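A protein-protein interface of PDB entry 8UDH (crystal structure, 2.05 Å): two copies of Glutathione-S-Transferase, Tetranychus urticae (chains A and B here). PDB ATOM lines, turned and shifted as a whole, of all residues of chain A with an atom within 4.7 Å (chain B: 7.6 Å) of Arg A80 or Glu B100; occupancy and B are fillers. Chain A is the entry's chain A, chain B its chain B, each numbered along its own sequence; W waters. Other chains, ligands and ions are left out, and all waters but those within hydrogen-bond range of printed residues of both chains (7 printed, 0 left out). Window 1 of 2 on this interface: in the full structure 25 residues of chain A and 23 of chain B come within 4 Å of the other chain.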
ATOM      1  N   VAL A  76     -23.531  -5.632 -13.520  1.00  0.00           N
ATOM      2  CA  VAL A  76     -22.144  -5.239 -13.139  1.00  0.00           C
ATOM      3  C   VAL A  76     -22.126  -3.776 -12.685  1.00  0.00           C
ATOM      4  O   VAL A  76     -21.453  -3.491 -11.699  1.00  0.00           O
ATOM      5  CB  VAL A  76     -21.141  -5.520 -14.278  1.00  0.00           C
ATOM      6  CG1 VAL A  76     -19.731  -5.076 -13.926  1.00  0.00           C
ATOM      7  CG2 VAL A  76     -21.157  -6.981 -14.695  1.00  0.00           C
ATOM      8  N   ALA A  77     -22.857  -2.904 -13.369  1.00  0.00           N
ATOM      9  CA  ALA A  77     -22.923  -1.527 -12.908  1.00  0.00           C
ATOM     10  C   ALA A  77     -23.550  -1.413 -11.510  1.00  0.00           C
ATOM     11  O   ALA A  77     -23.115  -0.589 -10.688  1.00  0.00           O
ATOM     12  CB  ALA A  77     -23.675  -0.684 -13.915  1.00  0.00           C
ATOM     13  N   ILE A  78     -24.588  -2.212 -11.244  1.00  0.00           N
ATOM     14  CA  ILE A  78     -25.242  -2.189  -9.950  1.00  0.00           C
ATOM     15  C   ILE A  78     -24.290  -2.710  -8.868  1.00  0.00           C
ATOM     16  O   ILE A  78     -24.170  -2.083  -7.819  1.00  0.00           O
ATOM     17  CB  ILE A  78     -26.551  -2.984  -9.942  1.00  0.00           C
ATOM     18  CG1 ILE A  78     -27.626  -2.389 -10.854  1.00  0.00           C
ATOM     19  CG2 ILE A  78     -27.078  -3.101  -8.509  1.00  0.00           C
ATOM     20  CD1 ILE A  78     -28.728  -3.349 -11.170  1.00  0.00           C
ATOM     21  N   ILE A  79     -23.636  -3.849  -9.106  1.00  0.00           N
ATOM     22  CA  ILE A  79     -22.838  -4.440  -8.060  1.00  0.00           C
ATOM     23  C   ILE A  79     -21.604  -3.562  -7.813  1.00  0.00           C
ATOM     24  O   ILE A  79     -21.192  -3.429  -6.677  1.00  0.00           O
ATOM     25  CB  ILE A  79     -22.498  -5.917  -8.331  1.00  0.00           C
ATOM     26  CG1 ILE A  79     -22.097  -6.595  -7.022  1.00  0.00           C
ATOM     27  CG2 ILE A  79     -21.391  -6.076  -9.372  1.00  0.00           C
ATOM     28  CD1 ILE A  79     -21.816  -8.071  -7.133  1.00  0.00           C
ATOM     29  N   ARG A  80     -21.020  -2.937  -8.838  1.00  0.00           N
ATOM     30  CA  ARG A  80     -19.888  -2.049  -8.617  1.00  0.00           C
ATOM     31  C   ARG A  80     -20.313  -0.810  -7.823  1.00  0.00           C
ATOM     32  O   ARG A  80     -19.581  -0.370  -6.930  1.00  0.00           O
ATOM     33  CB  ARG A  80     -19.198  -1.670  -9.940  1.00  0.00           C
ATOM     34  CG  ARG A  80     -18.448  -2.827 -10.600  1.00  0.00           C
ATOM     35  CD  ARG A  80     -17.793  -2.520 -11.944  1.00  0.00           C
ATOM     36  NE  ARG A  80     -16.899  -1.371 -11.928  1.00  0.00           N
ATOM     37  CZ  ARG A  80     -15.559  -1.435 -12.018  1.00  0.00           C
ATOM     38  NH1 ARG A  80     -14.951  -2.548 -11.639  1.00  0.00           N
ATOM     39  NH2 ARG A  80     -14.831  -0.403 -12.450  1.00  0.00           N
ATOM     40  N   TYR A  81     -21.467  -0.215  -8.153  1.00  0.00           N
ATOM     41  CA  TYR A  81     -22.023   0.885  -7.378  1.00  0.00           C
ATOM     42  C   TYR A  81     -22.136   0.499  -5.895  1.00  0.00           C
ATOM     43  O   TYR A  81     -21.751   1.276  -5.002  1.00  0.00           O
ATOM     44  CB  TYR A  81     -23.393   1.287  -7.945  1.00  0.00           C
ATOM     45  CG  TYR A  81     -24.172   2.189  -7.034  1.00  0.00           C
ATOM     46  CD1 TYR A  81     -23.907   3.546  -6.974  1.00  0.00           C
ATOM     47  CD2 TYR A  81     -25.145   1.670  -6.193  1.00  0.00           C
ATOM     48  CE1 TYR A  81     -24.605   4.370  -6.099  1.00  0.00           C
ATOM     49  CE2 TYR A  81     -25.829   2.470  -5.292  1.00  0.00           C
ATOM     50  CZ  TYR A  81     -25.544   3.823  -5.230  1.00  0.00           C
ATOM     51  OH  TYR A  81     -26.262   4.604  -4.354  1.00  0.00           O
ATOM     52  N   LEU A  82     -22.732  -0.681  -5.625  1.00  0.00           N
ATOM     53  CA  LEU A  82     -22.940  -1.119  -4.245  1.00  0.00           C
ATOM     54  C   LEU A  82     -21.601  -1.406  -3.573  1.00  0.00           C
ATOM     55  O   LEU A  82     -21.404  -1.101  -2.387  1.00  0.00           O
ATOM     56  CB  LEU A  82     -23.856  -2.347  -4.217  1.00  0.00           C
ATOM     57  CG  LEU A  82     -25.319  -2.053  -4.590  1.00  0.00           C
ATOM     58  CD1 LEU A  82     -26.096  -3.318  -4.753  1.00  0.00           C
ATOM     59  CD2 LEU A  82     -25.971  -1.150  -3.574  1.00  0.00           C
ATOM     60  N   ALA A  83     -20.660  -1.952  -4.356  1.00  0.00           N
ATOM     61  CA  ALA A  83     -19.331  -2.252  -3.827  1.00  0.00           C
ATOM     62  C   ALA A  83     -18.627  -0.965  -3.397  1.00  0.00           C
ATOM     63  O   ALA A  83     -18.044  -0.918  -2.321  1.00  0.00           O
ATOM     64  CB  ALA A  83     -18.509  -3.009  -4.832  1.00  0.00           C
ATOM     65  N   ARG A  84     -18.710   0.106  -4.193  1.00  0.00           N
ATOM     66  CA  ARG A  84     -18.051   1.348  -3.826  1.00  0.00           C
ATOM     67  C   ARG A  84     -18.673   1.947  -2.556  1.00  0.00           C
ATOM     68  O   ARG A  84     -17.957   2.443  -1.684  1.00  0.00           O
ATOM     69  CB  ARG A  84     -18.050   2.378  -4.954  1.00  0.00           C
ATOM     70  CG  ARG A  84     -17.270   1.917  -6.192  1.00  0.00           C
ATOM     71  CD  ARG A  84     -17.153   2.987  -7.285  1.00  0.00           C
ATOM     72  NE  ARG A  84     -18.490   3.328  -7.802  1.00  0.00           N
ATOM     73  CZ  ARG A  84     -19.086   2.779  -8.886  1.00  0.00           C
ATOM     74  NH1 ARG A  84     -18.512   1.787  -9.583  1.00  0.00           N
ATOM     75  NH2 ARG A  84     -20.279   3.250  -9.263  1.00  0.00           N
ATOM     76  N   GLU A 100     -10.770  -6.943 -11.107  1.00  0.00           N
ATOM     77  CA  GLU A 100     -11.400  -6.792 -12.442  1.00  0.00           C
ATOM     78  C   GLU A 100     -11.090  -8.001 -13.340  1.00  0.00           C
ATOM     79  O   GLU A 100     -11.976  -8.392 -14.096  1.00  0.00           O
ATOM     80  CB  GLU A 100     -11.026  -5.416 -12.994  1.00  0.00           C
ATOM     81  CG  GLU A 100     -11.700  -4.312 -12.206  1.00  0.00           C
ATOM     82  CD  GLU A 100     -11.459  -2.886 -12.657  1.00  0.00           C
ATOM     83  OE1 GLU A 100     -10.656  -2.685 -13.572  1.00  0.00           O
ATOM     84  OE2 GLU A 100     -12.097  -1.987 -12.095  1.00  0.00           O
ATOM     85  N   GLU A 103     -13.453 -10.603 -11.915  1.00  0.00           N
ATOM     86  CA  GLU A 103     -14.831 -10.195 -12.284  1.00  0.00           C
ATOM     87  C   GLU A 103     -15.135 -10.734 -13.683  1.00  0.00           C
ATOM     88  O   GLU A 103     -16.172 -11.368 -13.851  1.00  0.00           O
ATOM     89  CB  GLU A 103     -14.924  -8.667 -12.266  1.00  0.00           C
ATOM     90  CG  GLU A 103     -16.161  -8.088 -12.919  1.00  0.00           C
ATOM     91  CD  GLU A 103     -16.068  -6.595 -13.186  1.00  0.00           C
ATOM     92  OE1 GLU A 103     -15.998  -5.825 -12.222  1.00  0.00           O
ATOM     93  OE2 GLU A 103     -16.039  -6.214 -14.360  1.00  0.00           O
ATOM     94  N   TYR A 160     -16.323  -7.355  -3.766  1.00  0.00           N
ATOM     95  CA  TYR A 160     -17.566  -7.696  -4.451  1.00  0.00           C
ATOM     96  C   TYR A 160     -17.394  -8.898  -5.371  1.00  0.00           C
ATOM     97  O   TYR A 160     -18.342  -9.643  -5.601  1.00  0.00           O
ATOM     98  CB  TYR A 160     -18.141  -6.507  -5.203  1.00  0.00           C
ATOM     99  CG  TYR A 160     -17.374  -6.110  -6.437  1.00  0.00           C
ATOM    100  CD1 TYR A 160     -16.300  -5.243  -6.379  1.00  0.00           C
ATOM    101  CD2 TYR A 160     -17.753  -6.590  -7.675  1.00  0.00           C
ATOM    102  CE1 TYR A 160     -15.593  -4.897  -7.516  1.00  0.00           C
ATOM    103  CE2 TYR A 160     -17.086  -6.212  -8.830  1.00  0.00           C
ATOM    104  CZ  TYR A 160     -15.976  -5.396  -8.747  1.00  0.00           C
ATOM    105  OH  TYR A 160     -15.289  -5.027  -9.870  1.00  0.00           O
ATOM    106  N   VAL B  76     -11.936  -6.146 -20.600  1.00  0.00           N
ATOM    107  CA  VAL B  76     -12.509  -5.039 -19.777  1.00  0.00           C
ATOM    108  C   VAL B  76     -11.495  -4.596 -18.714  1.00  0.00           C
ATOM    109  O   VAL B  76     -11.348  -3.395 -18.531  1.00  0.00           O
ATOM    110  CB  VAL B  76     -13.880  -5.423 -19.183  1.00  0.00           C
ATOM    111  CG1 VAL B  76     -14.462  -4.307 -18.335  1.00  0.00           C
ATOM    112  CG2 VAL B  76     -14.863  -5.830 -20.268  1.00  0.00           C
ATOM    113  N   ARG B  80     -10.036  -0.741 -18.677  1.00  0.00           N
ATOM    114  CA  ARG B  80     -10.243   0.038 -17.426  1.00  0.00           C
ATOM    115  C   ARG B  80      -8.884   0.459 -16.840  1.00  0.00           C
ATOM    116  O   ARG B  80      -8.771   1.601 -16.408  1.00  0.00           O
ATOM    117  CB  ARG B  80     -11.089  -0.749 -16.423  1.00  0.00           C
ATOM    118  CG  ARG B  80     -12.531  -1.012 -16.833  1.00  0.00           C
ATOM    119  CD  ARG B  80     -13.333  -1.344 -15.589  1.00  0.00           C
ATOM    120  NE  ARG B  80     -14.648  -1.925 -15.807  1.00  0.00           N
ATOM    121  CZ  ARG B  80     -15.083  -3.030 -15.213  1.00  0.00           C
ATOM    122  NH1 ARG B  80     -14.251  -3.756 -14.489  1.00  0.00           N
ATOM    123  NH2 ARG B  80     -16.348  -3.399 -15.329  1.00  0.00           N
ATOM    124  N   ARG B  84      -7.925   4.422 -16.434  1.00  0.00           N
ATOM    125  CA  ARG B  84      -7.467   5.046 -15.168  1.00  0.00           C
ATOM    126  C   ARG B  84      -6.099   5.704 -15.396  1.00  0.00           C
ATOM    127  O   ARG B  84      -5.928   6.845 -14.982  1.00  0.00           O
ATOM    128  CB  ARG B  84      -7.429   4.004 -14.050  1.00  0.00           C
ATOM    129  CG  ARG B  84      -8.791   3.486 -13.617  1.00  0.00           C
ATOM    130  CD  ARG B  84      -8.704   2.503 -12.466  1.00  0.00           C
ATOM    131  NE  ARG B  84      -7.785   1.407 -12.727  1.00  0.00           N
ATOM    132  CZ  ARG B  84      -8.155   0.164 -13.005  1.00  0.00           C
ATOM    133  NH1 ARG B  84      -9.389  -0.083 -13.402  1.00  0.00           N
ATOM    134  NH2 ARG B  84      -7.284  -0.822 -12.910  1.00  0.00           N
ATOM    135  N   VAL B  89     -11.734   8.089 -17.298  1.00  0.00           N
ATOM    136  CA  VAL B  89     -12.777   7.495 -16.424  1.00  0.00           C
ATOM    137  C   VAL B  89     -13.661   8.617 -15.872  1.00  0.00           C
ATOM    138  O   VAL B  89     -13.400   9.774 -16.181  1.00  0.00           O
ATOM    139  CB  VAL B  89     -12.140   6.662 -15.295  1.00  0.00           C
ATOM    140  CG1 VAL B  89     -11.412   5.441 -15.827  1.00  0.00           C
ATOM    141  CG2 VAL B  89     -11.225   7.496 -14.416  1.00  0.00           C
ATOM    142  N   GLY B  90     -14.662   8.262 -15.072  1.00  0.00           N
ATOM    143  CA  GLY B  90     -15.576   9.257 -14.490  1.00  0.00           C
ATOM    144  C   GLY B  90     -14.911  10.149 -13.457  1.00  0.00           C
ATOM    145  O   GLY B  90     -14.020   9.667 -12.761  1.00  0.00           O
ATOM    146  N   ASP B  93     -19.325   9.990  -9.141  1.00  0.00           N
ATOM    147  CA  ASP B  93     -20.042   8.687  -9.157  1.00  0.00           C
ATOM    148  C   ASP B  93     -21.175   8.752 -10.172  1.00  0.00           C
ATOM    149  O   ASP B  93     -21.451   7.730 -10.779  1.00  0.00           O
ATOM    150  CB  ASP B  93     -20.617   8.246  -7.813  1.00  0.00           C
ATOM    151  CG  ASP B  93     -20.782   6.742  -7.662  1.00  0.00           C
ATOM    152  OD1 ASP B  93     -20.093   6.002  -8.378  1.00  0.00           O
ATOM    153  OD2 ASP B  93     -21.612   6.325  -6.834  1.00  0.00           O
ATOM    154  N   GLU B  94     -21.763   9.927 -10.353  1.00  0.00           N
ATOM    155  CA  GLU B  94     -22.813  10.059 -11.389  1.00  0.00           C
ATOM    156  C   GLU B  94     -22.206   9.669 -12.741  1.00  0.00           C
ATOM    157  O   GLU B  94     -22.791   8.832 -13.429  1.00  0.00           O
ATOM    158  CB  GLU B  94     -23.417  11.464 -11.399  1.00  0.00           C
ATOM    159  CG  GLU B  94     -24.404  11.677 -12.530  1.00  0.00           C
ATOM    160  CD  GLU B  94     -25.035  13.056 -12.601  1.00  0.00           C
ATOM    161  OE1 GLU B  94     -24.745  13.885 -11.721  1.00  0.00           O
ATOM    162  OE2 GLU B  94     -25.806  13.296 -13.549  1.00  0.00           O
ATOM    163  N   GLU B  95     -21.056  10.247 -13.067  1.00  0.00           N
ATOM    164  CA  GLU B  95     -20.390   9.927 -14.351  1.00  0.00           C
ATOM    165  C   GLU B  95     -20.040   8.435 -14.381  1.00  0.00           C
ATOM    166  O   GLU B  95     -20.293   7.805 -15.404  1.00  0.00           O
ATOM    167  CB  GLU B  95     -19.162  10.812 -14.536  1.00  0.00           C
ATOM    168  CG  GLU B  95     -19.475  12.219 -15.000  1.00  0.00           C
ATOM    169  CD  GLU B  95     -18.244  13.012 -15.407  1.00  0.00           C
ATOM    170  OE1 GLU B  95     -17.135  12.465 -15.319  1.00  0.00           O
ATOM    171  OE2 GLU B  95     -18.403  14.169 -15.813  1.00  0.00           O
ATOM    172  N   THR B  96     -19.527   7.903 -13.276  1.00  0.00           N
ATOM    173  CA  THR B  96     -19.067   6.486 -13.237  1.00  0.00           C
ATOM    174  C   THR B  96     -20.247   5.529 -13.486  1.00  0.00           C
ATOM    175  O   THR B  96     -20.086   4.612 -14.280  1.00  0.00           O
ATOM    176  CB  THR B  96     -18.257   6.219 -11.959  1.00  0.00           C
ATOM    177  OG1 THR B  96     -17.054   6.984 -12.015  1.00  0.00           O
ATOM    178  CG2 THR B  96     -17.932   4.755 -11.761  1.00  0.00           C
ATOM    179  N   ILE B  97     -21.391   5.771 -12.853  1.00  0.00           N
ATOM    180  CA  ILE B  97     -22.599   4.915 -13.044  1.00  0.00           C
ATOM    181  C   ILE B  97     -23.008   4.910 -14.524  1.00  0.00           C
ATOM    182  O   ILE B  97     -23.231   3.830 -15.065  1.00  0.00           O
ATOM    183  CB  ILE B  97     -23.736   5.387 -12.117  1.00  0.00           C
ATOM    184  CG1 ILE B  97     -23.372   5.217 -10.640  1.00  0.00           C
ATOM    185  CG2 ILE B  97     -25.042   4.688 -12.458  1.00  0.00           C
ATOM    186  CD1 ILE B  97     -24.322   5.904  -9.693  1.00  0.00           C
ATOM    187  N   LYS B  98     -23.049   6.080 -15.147  1.00  0.00           N
ATOM    188  CA  LYS B  98     -23.454   6.199 -16.568  1.00  0.00           C
ATOM    189  C   LYS B  98     -22.466   5.444 -17.459  1.00  0.00           C
ATOM    190  O   LYS B  98     -22.922   4.707 -18.324  1.00  0.00           O
ATOM    191  CB  LYS B  98     -23.522   7.681 -16.936  1.00  0.00           C
ATOM    192  CG  LYS B  98     -24.612   8.485 -16.245  1.00  0.00           C
ATOM    193  CD  LYS B  98     -24.639   9.927 -16.688  1.00  0.00           C
ATOM    194  CE  LYS B  98     -25.799  10.703 -16.105  1.00  0.00           C
ATOM    195  NZ  LYS B  98     -25.747  12.133 -16.485  1.00  0.00           N
ATOM    196  N   ILE B  99     -21.175   5.609 -17.205  1.00  0.00           N
ATOM    197  CA  ILE B  99     -20.102   4.948 -17.995  1.00  0.00           C
ATOM    198  C   ILE B  99     -20.239   3.430 -17.865  1.00  0.00           C
ATOM    199  O   ILE B  99     -20.200   2.762 -18.882  1.00  0.00           O
ATOM    200  CB  ILE B  99     -18.733   5.463 -17.500  1.00  0.00           C
ATOM    201  CG1 ILE B  99     -18.445   6.876 -18.015  1.00  0.00           C
ATOM    202  CG2 ILE B  99     -17.614   4.497 -17.850  1.00  0.00           C
ATOM    203  CD1 ILE B  99     -17.316   7.572 -17.301  1.00  0.00           C
ATOM    204  N   GLU B 100     -20.466   2.944 -16.653  1.00  0.00           N
ATOM    205  CA  GLU B 100     -20.536   1.484 -16.402  1.00  0.00           C
ATOM    206  C   GLU B 100     -21.820   0.884 -16.995  1.00  0.00           C
ATOM    207  O   GLU B 100     -21.753  -0.223 -17.519  1.00  0.00           O
ATOM    208  CB  GLU B 100     -20.300   1.256 -14.909  1.00  0.00           C
ATOM    209  CG  GLU B 100     -18.864   1.574 -14.535  1.00  0.00           C
ATOM    210  CD  GLU B 100     -18.419   1.336 -13.105  1.00  0.00           C
ATOM    211  OE1 GLU B 100     -19.256   0.950 -12.277  1.00  0.00           O
ATOM    212  OE2 GLU B 100     -17.226   1.526 -12.837  1.00  0.00           O
ATOM    213  N   MET B 101     -22.920   1.626 -16.959  1.00  0.00           N
ATOM    214  CA  MET B 101     -24.162   1.136 -17.603  1.00  0.00           C
ATOM    215  C   MET B 101     -23.920   0.994 -19.111  1.00  0.00           C
ATOM    216  O   MET B 101     -24.260  -0.051 -19.658  1.00  0.00           O
ATOM    217  CB  MET B 101     -25.325   2.093 -17.339  1.00  0.00           C
ATOM    218  CG  MET B 101     -26.021   1.850 -16.018  1.00  0.00           C
ATOM    219  SD  MET B 101     -27.602   2.715 -15.865  1.00  0.00           S
ATOM    220  CE  MET B 101     -27.118   4.393 -16.257  1.00  0.00           C
ATOM    221  N   VAL B 102     -23.315   2.004 -19.729  1.00  0.00           N
ATOM    222  CA  VAL B 102     -23.042   1.982 -21.197  1.00  0.00           C
ATOM    223  C   VAL B 102     -21.987   0.913 -21.509  1.00  0.00           C
ATOM    224  O   VAL B 102     -22.121   0.255 -22.530  1.00  0.00           O
ATOM    225  CB  VAL B 102     -22.648   3.375 -21.724  1.00  0.00           C
ATOM    226  CG1 VAL B 102     -22.218   3.333 -23.180  1.00  0.00           C
ATOM    227  CG2 VAL B 102     -23.764   4.386 -21.526  1.00  0.00           C
ATOM    228  N   GLU B 103     -20.986   0.754 -20.644  1.00  0.00           N
ATOM    229  CA  GLU B 103     -19.959  -0.300 -20.829  1.00  0.00           C
ATOM    230  C   GLU B 103     -20.677  -1.643 -20.976  1.00  0.00           C
ATOM    231  O   GLU B 103     -20.391  -2.357 -21.928  1.00  0.00           O
ATOM    232  CB  GLU B 103     -19.015  -0.309 -19.628  1.00  0.00           C
ATOM    233  CG  GLU B 103     -18.174  -1.562 -19.490  1.00  0.00           C
ATOM    234  CD  GLU B 103     -17.537  -1.731 -18.120  1.00  0.00           C
ATOM    235  OE1 GLU B 103     -16.703  -0.895 -17.748  1.00  0.00           O
ATOM    236  OE2 GLU B 103     -17.892  -2.691 -17.425  1.00  0.00           O
ATOM    237  N   GLN B 104     -21.608  -1.923 -20.073  1.00  0.00           N
ATOM    238  CA  GLN B 104     -22.346  -3.211 -20.067  1.00  0.00           C
ATOM    239  C   GLN B 104     -23.277  -3.312 -21.284  1.00  0.00           C
ATOM    240  O   GLN B 104     -23.348  -4.385 -21.871  1.00  0.00           O
ATOM    241  CB  GLN B 104     -23.066  -3.327 -18.726  1.00  0.00           C
ATOM    242  CG  GLN B 104     -22.104  -3.379 -17.551  1.00  0.00           C
ATOM    243  CD  GLN B 104     -21.244  -4.611 -17.651  1.00  0.00           C
ATOM    244  OE1 GLN B 104     -21.753  -5.723 -17.716  1.00  0.00           O
ATOM    245  NE2 GLN B 104     -19.936  -4.424 -17.680  1.00  0.00           N
ATOM    246  N   GLN B 105     -23.916  -2.211 -21.661  1.00  0.00           N
ATOM    247  CA  GLN B 105     -24.808  -2.206 -22.849  1.00  0.00           C
ATOM    248  C   GLN B 105     -23.984  -2.487 -24.112  1.00  0.00           C
ATOM    249  O   GLN B 105     -24.428  -3.295 -24.924  1.00  0.00           O
ATOM    250  CB  GLN B 105     -25.585  -0.891 -22.927  1.00  0.00           C
ATOM    251  CG  GLN B 105     -26.621  -0.871 -24.040  1.00  0.00           C
ATOM    252  CD  GLN B 105     -27.687  -1.919 -23.841  1.00  0.00           C
ATOM    253  OE1 GLN B 105     -28.484  -1.852 -22.910  1.00  0.00           O
ATOM    254  NE2 GLN B 105     -27.717  -2.897 -24.731  1.00  0.00           N
ATOM    255  N   ALA B 106     -22.809  -1.869 -24.230  1.00  0.00           N
ATOM    256  CA  ALA B 106     -21.928  -2.089 -25.395  1.00  0.00           C
ATOM    257  C   ALA B 106     -21.484  -3.553 -25.445  1.00  0.00           C
ATOM    258  O   ALA B 106     -21.528  -4.133 -26.526  1.00  0.00           O
ATOM    259  CB  ALA B 106     -20.750  -1.162 -25.316  1.00  0.00           C
ATOM    260  N   ILE B 107     -21.076  -4.108 -24.307  1.00  0.00           N
ATOM    261  CA  ILE B 107     -20.617  -5.526 -24.235  1.00  0.00           C
ATOM    262  C   ILE B 107     -21.766  -6.462 -24.626  1.00  0.00           C
ATOM    263  O   ILE B 107     -21.507  -7.408 -25.357  1.00  0.00           O
ATOM    264  CB  ILE B 107     -20.056  -5.835 -22.833  1.00  0.00           C
ATOM    265  CG1 ILE B 107     -18.806  -5.008 -22.529  1.00  0.00           C
ATOM    266  CG2 ILE B 107     -19.788  -7.321 -22.675  1.00  0.00           C
ATOM    267  CD1 ILE B 107     -18.357  -5.084 -21.093  1.00  0.00           C
ATOM    268  N   ILE B 153     -20.693  10.010 -24.260  1.00  0.00           N
ATOM    269  CA  ILE B 153     -21.587   9.420 -23.216  1.00  0.00           C
ATOM    270  C   ILE B 153     -21.778  10.352 -22.009  1.00  0.00           C
ATOM    271  O   ILE B 153     -22.914  10.493 -21.572  1.00  0.00           O
ATOM    272  CB  ILE B 153     -21.074   8.017 -22.822  1.00  0.00           C
ATOM    273  CG1 ILE B 153     -21.190   7.043 -23.995  1.00  0.00           C
ATOM    274  CG2 ILE B 153     -21.780   7.498 -21.580  1.00  0.00           C
ATOM    275  CD1 ILE B 153     -22.558   7.020 -24.630  1.00  0.00           C
ATOM    276  N   ILE B 154     -20.719  10.969 -21.493  1.00  0.00           N
ATOM    277  CA  ILE B 154     -20.878  11.810 -20.268  1.00  0.00           C
ATOM    278  C   ILE B 154     -20.766  13.293 -20.649  1.00  0.00           C
ATOM    279  O   ILE B 154     -20.516  14.111 -19.755  1.00  0.00           O
ATOM    280  CB  ILE B 154     -19.913  11.391 -19.135  1.00  0.00           C
ATOM    281  CG1 ILE B 154     -18.460  11.296 -19.606  1.00  0.00           C
ATOM    282  CG2 ILE B 154     -20.378  10.097 -18.488  1.00  0.00           C
ATOM    283  CD1 ILE B 154     -17.656  12.546 -19.383  1.00  0.00           C
ATOM    284  N   TYR B 160     -13.494   6.013 -21.890  1.00  0.00           N
ATOM    285  CA  TYR B 160     -13.131   4.707 -22.502  1.00  0.00           C
ATOM    286  C   TYR B 160     -14.349   4.026 -23.139  1.00  0.00           C
ATOM    287  O   TYR B 160     -14.166   3.352 -24.147  1.00  0.00           O
ATOM    288  CB  TYR B 160     -12.454   3.805 -21.468  1.00  0.00           C
ATOM    289  CG  TYR B 160     -13.338   3.209 -20.406  1.00  0.00           C
ATOM    290  CD1 TYR B 160     -13.584   3.879 -19.221  1.00  0.00           C
ATOM    291  CD2 TYR B 160     -13.903   1.957 -20.573  1.00  0.00           C
ATOM    292  CE1 TYR B 160     -14.382   3.328 -18.236  1.00  0.00           C
ATOM    293  CE2 TYR B 160     -14.705   1.391 -19.599  1.00  0.00           C
ATOM    294  CZ  TYR B 160     -14.945   2.081 -18.426  1.00  0.00           C
ATOM    295  OH  TYR B 160     -15.736   1.531 -17.459  1.00  0.00           O
ATOM    296  N   VAL B 161     -15.530   4.203 -22.553  1.00  0.00           N
ATOM    297  CA  VAL B 161     -16.766   3.534 -23.053  1.00  0.00           C
ATOM    298  C   VAL B 161     -17.079   4.009 -24.473  1.00  0.00           C
ATOM    299  O   VAL B 161     -17.675   3.240 -25.217  1.00  0.00           O
ATOM    300  CB  VAL B 161     -17.961   3.740 -22.104  1.00  0.00           C
ATOM    301  CG1 VAL B 161     -17.852   2.849 -20.883  1.00  0.00           C
ATOM    302  CG2 VAL B 161     -18.161   5.193 -21.711  1.00  0.00           C
HETATM  303  O   HOH W   1      -8.226  -3.249 -14.400  1.00  0.00           O
HETATM  304  O   HOH W   2     -15.519   2.260 -10.755  1.00  0.00           O
HETATM  305  O   HOH W   3     -17.567   6.490  -7.761  1.00  0.00           O
HETATM  306  O   HOH W   4     -21.076   4.094  -5.372  1.00  0.00           O
HETATM  307  O   HOH W   5     -11.788   0.594 -12.033  1.00  0.00           O
HETATM  308  O   HOH W   6     -21.677   1.640 -11.401  1.00  0.00           O
HETATM  309  O   HOH W   7     -23.939  -6.054 -16.487  1.00  0.00           O
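NH1 of Arg A80 is in hydrogen-bond range of OH of Tyr A160 (3.1 Å). The side-chain carboxylate (OE2) of Glu B103 is in hydrogen-bond range of the side-chain amide nitrogen (NE2) of Gln B104, 2.7 Å away. The side-chain hydroxyl (OH) of Tyr A160 is in hydrogen-bond range of the side-chain carboxylate (OE1) of Glu A103.
The guanidinium group (NH1) of Arg B80 lies close to the guanidinium group (NH1) of Arg A80 (3.2 Å). OE2 of Glu A100 lies within salt-bridge range of NH1 of Arg B80 (3.7 Å). The guanidinium group (NE) of Arg A80 lies within salt-bridge range of the side-chain carboxylate (OE2) of Glu B100, 3.1 Å away. OE1 of Glu A100 is in salt-bridge range of NH1 of Arg B84, 2.9 Å away. The guanidinium group of Arg A84 lies within salt-bridge range of the side-chain carboxylate of Glu B100. The side-chain carboxylate (OE2) of Glu A103 lies within salt-bridge range of the guanidinium group (NH2) of Arg B80 (3.0 Å). The guanidinium group of Arg A84 lies within salt-bridge range of the side-chain carboxylate of Asp B93.
Printed residues of chain A that touch a printed residue of chain B: Val A76, Ala A77, Arg A80, Tyr A81, Arg A84, Glu A100 and Glu A103. Hydrophobic or aromatic side chains of chain A within 4 Å of the printed part of chain B: Val A76, Ala A77 and Tyr A81. Among the printed residues, 14 pairs touch across the chains. Among the printed residues, Asp or Glu carboxylates within 4 Å of a Lys or Arg side-chain nitrogen of the other chain: Arg A80 with Glu B100, Arg A84 with Asp B93, Arg A84 with Glu B100, Glu A100 with Arg B80, Glu A100 with Arg B84 and Glu A103 with Arg B80.
Of chain B, only Arg B80 (3.2 Å) and Glu B100 (3.1 Å) come within 4 Å of Arg A80. Glu B100 touches three residues of chain A. Of the printed residues of chain A, Ile B97 touches Tyr A81 and Arg A84. Printed residues of chain B within 4 Å of Val A76: Gln B104. Of the printed residues of chain A, Thr B96 touches Arg A84 (3.7 Å). Glu B95 touches none of the printed residues of chain A. The nearest printed residue of chain A that does not touch Glu B100 is Tyr A81 (4.8 Å). The nearest printed residue of chain B that does not touch Glu A103 is Val B76 (4.7 Å).
CG2 of Val A76 touches OE1 of Gln B104, at 3.3 Å. C of Glu B100 touches CB of Ala A77, at 3.9 Å. CB of Ala A77 touches N of Met B101, 3.9 Å away. Tyr A81 touches Asp B93 (CD1 to OD2, 3.6 Å). Ile B97 touches Tyr A81 (CD1 to CD1, 3.6 Å). Arg A84 touches Thr B96. Arg A84 touches Ile B97 (NH2 to CG1, 3.9 Å).
Water W7 bridges OE1 of Gln B104 (2.5 Å) and N of Val A76 (3.0 Å). Water W6 lies within hydrogen-bond range of the side-chain carboxylate of Glu B100 (2.7 Å), the backbone carbonyl oxygen of Ala A77 (2.7 Å) and the guanidinium group of Arg A84 (3.0 Å).
Arg A84 touches Glu B100, and with the chains exchanged Glu A100 touches Arg B84. Glu A103 touches Arg B80, but with the chains exchanged Arg A80 does not touch Glu B103 (5.5 Å). Of the 14 pairs that touch across the chains among the printed residues, 5 have their exchanged pair printed and touching as well.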
